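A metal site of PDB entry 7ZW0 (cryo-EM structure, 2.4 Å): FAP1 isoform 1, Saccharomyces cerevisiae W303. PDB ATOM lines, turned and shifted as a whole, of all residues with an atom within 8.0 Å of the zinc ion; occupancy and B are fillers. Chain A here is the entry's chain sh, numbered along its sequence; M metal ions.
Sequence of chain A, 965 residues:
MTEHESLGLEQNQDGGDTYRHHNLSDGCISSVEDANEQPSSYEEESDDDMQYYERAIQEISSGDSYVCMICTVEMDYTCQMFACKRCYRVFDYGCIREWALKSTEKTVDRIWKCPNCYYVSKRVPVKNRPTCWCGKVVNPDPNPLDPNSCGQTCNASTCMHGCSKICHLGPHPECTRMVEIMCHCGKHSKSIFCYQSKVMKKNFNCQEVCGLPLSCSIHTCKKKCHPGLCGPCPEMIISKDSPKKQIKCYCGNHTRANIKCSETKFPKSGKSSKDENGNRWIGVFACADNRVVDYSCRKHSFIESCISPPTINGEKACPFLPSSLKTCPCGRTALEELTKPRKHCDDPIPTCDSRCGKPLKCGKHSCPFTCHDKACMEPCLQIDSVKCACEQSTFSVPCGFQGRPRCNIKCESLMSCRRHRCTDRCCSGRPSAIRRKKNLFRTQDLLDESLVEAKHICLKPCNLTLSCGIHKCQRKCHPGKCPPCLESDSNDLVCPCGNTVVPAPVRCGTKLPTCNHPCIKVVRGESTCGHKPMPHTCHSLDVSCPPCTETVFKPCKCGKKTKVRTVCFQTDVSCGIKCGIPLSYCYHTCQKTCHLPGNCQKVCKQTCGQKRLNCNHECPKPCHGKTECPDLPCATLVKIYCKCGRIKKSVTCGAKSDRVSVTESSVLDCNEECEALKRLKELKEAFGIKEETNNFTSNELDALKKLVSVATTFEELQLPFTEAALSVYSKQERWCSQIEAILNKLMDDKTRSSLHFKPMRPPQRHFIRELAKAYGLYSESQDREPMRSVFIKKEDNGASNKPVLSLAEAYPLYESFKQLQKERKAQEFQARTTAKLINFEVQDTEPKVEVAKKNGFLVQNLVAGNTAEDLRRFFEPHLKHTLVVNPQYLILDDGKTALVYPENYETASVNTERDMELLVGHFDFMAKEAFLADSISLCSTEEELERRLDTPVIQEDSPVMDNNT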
ATOM      1  N   MET A  69     -17.714   9.029 -27.228  1.00  0.00           N
ATOM      2  CA  MET A  69     -18.411   7.788 -27.567  1.00  0.00           C
ATOM      3  C   MET A  69     -19.215   7.119 -26.461  1.00  0.00           C
ATOM      4  O   MET A  69     -20.332   6.667 -26.704  1.00  0.00           O
ATOM      5  CB  MET A  69     -17.427   6.787 -28.173  1.00  0.00           C
ATOM      6  CG  MET A  69     -16.825   7.256 -29.484  1.00  0.00           C
ATOM      7  SD  MET A  69     -15.799   6.014 -30.300  1.00  0.00           S
ATOM      8  CE  MET A  69     -17.010   4.737 -30.626  1.00  0.00           C
ATOM      9  N   PHE A  82      -9.641  11.904 -24.099  1.00  0.00           N
ATOM     10  CA  PHE A  82      -8.696  10.779 -24.030  1.00  0.00           C
ATOM     11  C   PHE A  82      -8.363  10.266 -25.433  1.00  0.00           C
ATOM     12  O   PHE A  82      -9.268  10.103 -26.254  1.00  0.00           O
ATOM     13  CB  PHE A  82      -9.269   9.644 -23.208  1.00  0.00           C
ATOM     14  CG  PHE A  82      -8.380   8.431 -23.158  1.00  0.00           C
ATOM     15  CD1 PHE A  82      -7.265   8.419 -22.345  1.00  0.00           C
ATOM     16  CD2 PHE A  82      -8.670   7.312 -23.909  1.00  0.00           C
ATOM     17  CE1 PHE A  82      -6.436   7.309 -22.291  1.00  0.00           C
ATOM     18  CE2 PHE A  82      -7.851   6.204 -23.875  1.00  0.00           C
ATOM     19  CZ  PHE A  82      -6.741   6.199 -23.058  1.00  0.00           C
ATOM     20  N   ALA A  83      -7.092  10.030 -25.714  1.00  0.00           N
ATOM     21  CA  ALA A  83      -6.692   9.601 -27.049  1.00  0.00           C
ATOM     22  C   ALA A  83      -6.073   8.220 -27.054  1.00  0.00           C
ATOM     23  O   ALA A  83      -5.262   7.891 -26.189  1.00  0.00           O
ATOM     24  CB  ALA A  83      -5.755  10.612 -27.670  1.00  0.00           C
ATOM     25  N   CYS A  84      -6.439   7.407 -28.031  1.00  0.00           N
ATOM     26  CA  CYS A  84      -5.847   6.082 -28.156  1.00  0.00           C
ATOM     27  C   CYS A  84      -5.103   6.031 -29.468  1.00  0.00           C
ATOM     28  O   CYS A  84      -5.643   6.434 -30.487  1.00  0.00           O
ATOM     29  CB  CYS A  84      -6.912   4.986 -28.111  1.00  0.00           C
ATOM     30  SG  CYS A  84      -6.294   3.338 -28.495  1.00  0.00           S
ATOM     31  N   LYS A  85      -3.873   5.545 -29.461  1.00  0.00           N
ATOM     32  CA  LYS A  85      -3.080   5.551 -30.679  1.00  0.00           C
ATOM     33  C   LYS A  85      -3.698   4.694 -31.763  1.00  0.00           C
ATOM     34  O   LYS A  85      -3.692   5.062 -32.928  1.00  0.00           O
ATOM     35  CB  LYS A  85      -1.644   5.077 -30.391  1.00  0.00           C
ATOM     36  CG  LYS A  85      -0.739   6.126 -29.744  1.00  0.00           C
ATOM     37  CD  LYS A  85      -0.948   6.229 -28.237  1.00  0.00           C
ATOM     38  CE  LYS A  85      -1.648   7.515 -27.858  1.00  0.00           C
ATOM     39  NZ  LYS A  85      -2.144   7.477 -26.455  1.00  0.00           N
ATOM     40  N   ARG A  86      -4.249   3.549 -31.387  1.00  0.00           N
ATOM     41  CA  ARG A  86      -4.800   2.642 -32.381  1.00  0.00           C
ATOM     42  C   ARG A  86      -5.978   3.253 -33.151  1.00  0.00           C
ATOM     43  O   ARG A  86      -6.049   3.127 -34.376  1.00  0.00           O
ATOM     44  CB  ARG A  86      -5.202   1.315 -31.726  1.00  0.00           C
ATOM     45  CG  ARG A  86      -5.382   0.172 -32.716  1.00  0.00           C
ATOM     46  CD  ARG A  86      -4.082  -0.144 -33.430  1.00  0.00           C
ATOM     47  NE  ARG A  86      -4.296  -0.918 -34.648  1.00  0.00           N
ATOM     48  CZ  ARG A  86      -4.445  -0.386 -35.859  1.00  0.00           C
ATOM     49  NH1 ARG A  86      -4.395   0.926 -36.014  1.00  0.00           N
ATOM     50  NH2 ARG A  86      -4.645  -1.167 -36.914  1.00  0.00           N
ATOM     51  N   CYS A  87      -6.880   3.925 -32.449  1.00  0.00           N
ATOM     52  CA  CYS A  87      -8.028   4.535 -33.118  1.00  0.00           C
ATOM     53  C   CYS A  87      -7.886   6.018 -33.386  1.00  0.00           C
ATOM     54  O   CYS A  87      -8.691   6.578 -34.131  1.00  0.00           O
ATOM     55  CB  CYS A  87      -9.286   4.328 -32.286  1.00  0.00           C
ATOM     56  SG  CYS A  87      -9.318   5.303 -30.767  1.00  0.00           S
ATOM     57  N   TYR A  88      -6.869   6.652 -32.827  1.00  0.00           N
ATOM     58  CA  TYR A  88      -6.721   8.104 -32.946  1.00  0.00           C
ATOM     59  C   TYR A  88      -8.054   8.839 -32.872  1.00  0.00           C
ATOM     60  O   TYR A  88      -8.335   9.721 -33.692  1.00  0.00           O
ATOM     61  CB  TYR A  88      -5.912   8.490 -34.185  1.00  0.00           C
ATOM     62  CG  TYR A  88      -4.427   8.380 -33.945  1.00  0.00           C
ATOM     63  CD1 TYR A  88      -3.851   8.986 -32.834  1.00  0.00           C
ATOM     64  CD2 TYR A  88      -3.609   7.692 -34.819  1.00  0.00           C
ATOM     65  CE1 TYR A  88      -2.492   8.891 -32.601  1.00  0.00           C
ATOM     66  CE2 TYR A  88      -2.252   7.588 -34.596  1.00  0.00           C
ATOM     67  CZ  TYR A  88      -1.697   8.185 -33.476  1.00  0.00           C
ATOM     68  OH  TYR A  88      -0.345   8.089 -33.249  1.00  0.00           O
ATOM     69  N   ARG A  89      -8.873   8.494 -31.885  1.00  0.00           N
ATOM     70  CA  ARG A  89     -10.162   9.128 -31.711  1.00  0.00           C
ATOM     71  C   ARG A  89     -10.241   9.630 -30.274  1.00  0.00           C
ATOM     72  O   ARG A  89      -9.544   9.110 -29.399  1.00  0.00           O
ATOM     73  CB  ARG A  89     -11.271   8.117 -32.025  1.00  0.00           C
ATOM     74  CG  ARG A  89     -12.643   8.383 -31.428  1.00  0.00           C
ATOM     75  CD  ARG A  89     -13.613   8.935 -32.455  1.00  0.00           C
ATOM     76  NE  ARG A  89     -14.884   9.315 -31.847  1.00  0.00           N
ATOM     77  CZ  ARG A  89     -15.945   9.752 -32.528  1.00  0.00           C
ATOM     78  NH1 ARG A  89     -15.884   9.846 -33.848  1.00  0.00           N
ATOM     79  NH2 ARG A  89     -17.053  10.089 -31.886  1.00  0.00           N
ATOM     80  N   VAL A  90     -11.067  10.630 -30.008  1.00  0.00           N
ATOM     81  CA  VAL A  90     -11.157  11.201 -28.666  1.00  0.00           C
ATOM     82  C   VAL A  90     -12.514  11.065 -27.986  1.00  0.00           C
ATOM     83  O   VAL A  90     -13.561  11.244 -28.624  1.00  0.00           O
ATOM     84  CB  VAL A  90     -10.674  12.657 -28.664  1.00  0.00           C
ATOM     85  CG1 VAL A  90     -11.340  13.482 -27.591  1.00  0.00           C
ATOM     86  CG2 VAL A  90      -9.170  12.692 -28.515  1.00  0.00           C
ATOM     87  N   PHE A  91     -12.517  10.695 -26.708  1.00  0.00           N
ATOM     88  CA  PHE A  91     -13.761  10.569 -25.957  1.00  0.00           C
ATOM     89  C   PHE A  91     -13.567  11.391 -24.702  1.00  0.00           C
ATOM     90  O   PHE A  91     -12.458  11.814 -24.415  1.00  0.00           O
ATOM     91  CB  PHE A  91     -14.006   9.110 -25.575  1.00  0.00           C
ATOM     92  CG  PHE A  91     -13.171   8.132 -26.341  1.00  0.00           C
ATOM     93  CD1 PHE A  91     -11.896   7.791 -25.894  1.00  0.00           C
ATOM     94  CD2 PHE A  91     -13.647   7.549 -27.504  1.00  0.00           C
ATOM     95  CE1 PHE A  91     -11.121   6.888 -26.605  1.00  0.00           C
ATOM     96  CE2 PHE A  91     -12.881   6.647 -28.204  1.00  0.00           C
ATOM     97  CZ  PHE A  91     -11.608   6.321 -27.760  1.00  0.00           C
ATOM     98  N   ILE A  96     -14.664   7.607 -20.723  1.00  0.00           N
ATOM     99  CA  ILE A  96     -13.920   6.444 -21.167  1.00  0.00           C
ATOM    100  C   ILE A  96     -13.345   5.664 -19.976  1.00  0.00           C
ATOM    101  O   ILE A  96     -13.189   4.446 -20.061  1.00  0.00           O
ATOM    102  CB  ILE A  96     -12.821   6.819 -22.189  1.00  0.00           C
ATOM    103  CG1 ILE A  96     -12.434   5.607 -23.042  1.00  0.00           C
ATOM    104  CG2 ILE A  96     -11.575   7.375 -21.508  1.00  0.00           C
ATOM    105  CD1 ILE A  96     -13.576   5.052 -23.860  1.00  0.00           C
ATOM    106  N   TRP A 112      -8.837  -3.190 -20.113  1.00  0.00           N
ATOM    107  CA  TRP A 112      -9.755  -2.186 -20.645  1.00  0.00           C
ATOM    108  C   TRP A 112      -9.799  -2.198 -22.179  1.00  0.00           C
ATOM    109  O   TRP A 112      -8.804  -2.503 -22.816  1.00  0.00           O
ATOM    110  CB  TRP A 112      -9.379  -0.801 -20.117  1.00  0.00           C
ATOM    111  CG  TRP A 112      -8.638   0.059 -21.080  1.00  0.00           C
ATOM    112  CD1 TRP A 112      -7.301   0.051 -21.332  1.00  0.00           C
ATOM    113  CD2 TRP A 112      -9.200   1.081 -21.927  1.00  0.00           C
ATOM    114  NE1 TRP A 112      -6.999   1.000 -22.276  1.00  0.00           N
ATOM    115  CE2 TRP A 112      -8.147   1.638 -22.660  1.00  0.00           C
ATOM    116  CE3 TRP A 112     -10.497   1.563 -22.128  1.00  0.00           C
ATOM    117  CZ2 TRP A 112      -8.339   2.656 -23.580  1.00  0.00           C
ATOM    118  CZ3 TRP A 112     -10.681   2.569 -23.039  1.00  0.00           C
ATOM    119  CH2 TRP A 112      -9.619   3.114 -23.762  1.00  0.00           C
ATOM    120  N   LYS A 113     -10.944  -1.856 -22.777  1.00  0.00           N
ATOM    121  CA  LYS A 113     -11.060  -1.929 -24.248  1.00  0.00           C
ATOM    122  C   LYS A 113     -11.403  -0.588 -24.884  1.00  0.00           C
ATOM    123  O   LYS A 113     -12.238   0.137 -24.369  1.00  0.00           O
ATOM    124  CB  LYS A 113     -12.116  -2.970 -24.638  1.00  0.00           C
ATOM    125  CG  LYS A 113     -12.135  -3.302 -26.123  1.00  0.00           C
ATOM    126  CD  LYS A 113     -12.827  -4.628 -26.371  1.00  0.00           C
ATOM    127  CE  LYS A 113     -12.516  -5.134 -27.768  1.00  0.00           C
ATOM    128  NZ  LYS A 113     -13.043  -6.516 -27.979  1.00  0.00           N
ATOM    129  N   CYS A 114     -10.770  -0.269 -25.994  1.00  0.00           N
ATOM    130  CA  CYS A 114     -11.082   0.963 -26.690  1.00  0.00           C
ATOM    131  C   CYS A 114     -12.089   0.684 -27.783  1.00  0.00           C
ATOM    132  O   CYS A 114     -11.809  -0.087 -28.693  1.00  0.00           O
ATOM    133  CB  CYS A 114      -9.824   1.579 -27.284  1.00  0.00           C
ATOM    134  SG  CYS A 114     -10.125   3.150 -28.114  1.00  0.00           S
ATOM    135  N   PRO A 115     -13.265   1.317 -27.726  1.00  0.00           N
ATOM    136  CA  PRO A 115     -14.341   1.026 -28.686  1.00  0.00           C
ATOM    137  C   PRO A 115     -14.102   1.365 -30.156  1.00  0.00           C
ATOM    138  O   PRO A 115     -14.479   0.558 -31.006  1.00  0.00           O
ATOM    139  CB  PRO A 115     -15.511   1.881 -28.183  1.00  0.00           C
ATOM    140  CG  PRO A 115     -15.162   2.249 -26.771  1.00  0.00           C
ATOM    141  CD  PRO A 115     -13.672   2.334 -26.739  1.00  0.00           C
ATOM    142  N   ASN A 116     -13.508   2.505 -30.459  1.00  0.00           N
ATOM    143  CA  ASN A 116     -13.372   2.895 -31.866  1.00  0.00           C
ATOM    144  C   ASN A 116     -12.515   1.935 -32.660  1.00  0.00           C
ATOM    145  O   ASN A 116     -12.853   1.581 -33.794  1.00  0.00           O
ATOM    146  CB  ASN A 116     -12.834   4.321 -31.986  1.00  0.00           C
ATOM    147  CG  ASN A 116     -13.124   4.934 -33.352  1.00  0.00           C
ATOM    148  OD1 ASN A 116     -14.276   4.956 -33.793  1.00  0.00           O
ATOM    149  ND2 ASN A 116     -12.094   5.445 -34.004  1.00  0.00           N
ATOM    150  N   CYS A 117     -11.408   1.492 -32.084  1.00  0.00           N
ATOM    151  CA  CYS A 117     -10.567   0.510 -32.753  1.00  0.00           C
ATOM    152  C   CYS A 117     -10.946  -0.880 -32.309  1.00  0.00           C
ATOM    153  O   CYS A 117     -10.334  -1.855 -32.758  1.00  0.00           O
ATOM    154  CB  CYS A 117      -9.097   0.769 -32.455  1.00  0.00           C
ATOM    155  SG  CYS A 117      -8.772   1.160 -30.731  1.00  0.00           S
ATOM    156  N   TYR A 118     -11.930  -0.985 -31.423  1.00  0.00           N
ATOM    157  CA  TYR A 118     -12.333  -2.281 -30.879  1.00  0.00           C
ATOM    158  C   TYR A 118     -11.070  -2.993 -30.447  1.00  0.00           C
ATOM    159  O   TYR A 118     -10.880  -4.171 -30.740  1.00  0.00           O
ATOM    160  CB  TYR A 118     -13.117  -3.097 -31.921  1.00  0.00           C
ATOM    161  CG  TYR A 118     -14.021  -4.139 -31.325  1.00  0.00           C
ATOM    162  CD1 TYR A 118     -15.045  -3.789 -30.451  1.00  0.00           C
ATOM    163  CD2 TYR A 118     -13.864  -5.483 -31.639  1.00  0.00           C
ATOM    164  CE1 TYR A 118     -15.870  -4.744 -29.903  1.00  0.00           C
ATOM    165  CE2 TYR A 118     -14.691  -6.448 -31.101  1.00  0.00           C
ATOM    166  CZ  TYR A 118     -15.701  -6.069 -30.235  1.00  0.00           C
ATOM    167  OH  TYR A 118     -16.533  -7.026 -29.693  1.00  0.00           O
ATOM    168  N   TYR A 119     -10.192  -2.278 -29.753  1.00  0.00           N
ATOM    169  CA  TYR A 119      -8.911  -2.858 -29.362  1.00  0.00           C
ATOM    170  C   TYR A 119      -8.730  -2.826 -27.872  1.00  0.00           C
ATOM    171  O   TYR A 119      -8.883  -1.780 -27.244  1.00  0.00           O
ATOM    172  CB  TYR A 119      -7.777  -2.136 -30.106  1.00  0.00           C
ATOM    173  CG  TYR A 119      -6.536  -1.783 -29.305  1.00  0.00           C
ATOM    174  CD1 TYR A 119      -6.433  -0.574 -28.635  1.00  0.00           C
ATOM    175  CD2 TYR A 119      -5.445  -2.640 -29.270  1.00  0.00           C
ATOM    176  CE1 TYR A 119      -5.306  -0.241 -27.916  1.00  0.00           C
ATOM    177  CE2 TYR A 119      -4.313  -2.313 -28.555  1.00  0.00           C
ATOM    178  CZ  TYR A 119      -4.249  -1.122 -27.883  1.00  0.00           C
ATOM    179  OH  TYR A 119      -3.122  -0.788 -27.164  1.00  0.00           O
ATOM    180  N   VAL A 120      -8.438  -3.977 -27.281  1.00  0.00           N
ATOM    181  CA  VAL A 120      -8.198  -4.021 -25.847  1.00  0.00           C
ATOM    182  C   VAL A 120      -6.808  -3.526 -25.517  1.00  0.00           C
ATOM    183  O   VAL A 120      -5.868  -3.761 -26.263  1.00  0.00           O
ATOM    184  CB  VAL A 120      -8.357  -5.452 -25.312  1.00  0.00           C
ATOM    185  CG1 VAL A 120      -9.439  -5.498 -24.238  1.00  0.00           C
ATOM    186  CG2 VAL A 120      -8.695  -6.397 -26.442  1.00  0.00           C
ATOM    187  N   SER A 121      -6.664  -2.853 -24.389  1.00  0.00           N
ATOM    188  CA  SER A 121      -5.349  -2.396 -23.942  1.00  0.00           C
ATOM    189  C   SER A 121      -5.205  -2.808 -22.496  1.00  0.00           C
ATOM    190  O   SER A 121      -6.202  -3.175 -21.861  1.00  0.00           O
ATOM    191  CB  SER A 121      -5.174  -0.892 -24.148  1.00  0.00           C
ATOM    192  OG  SER A 121      -3.860  -0.475 -23.806  1.00  0.00           O
HETATM  193 ZN    ZN M   1      -8.618   3.428 -29.472  1.00  0.00          ZN
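O of Tyr 119 sits at hydrogen-bond distance from N of Cys 114 (2.7 Å). The side-chain sulfur (SG) of Cys 87 lies close to the backbone NH (N) of Arg 89 (3.4 Å). SG of Cys 84 lies close to N of Arg 86.
Of the 22 residues printed, 4 come within 4 Å of the zinc ion.
The zinc ion is bound by the side-chain sulfur (SG) of Cys 114, 2.0 Å away. SG of Cys 87 binds the zinc ion (2.4 Å). The side-chain sulfur (SG) of Cys 84 is bound to the zinc ion (2.5 Å). The zinc ion is bound by SG of Cys 117 (2.6 Å).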
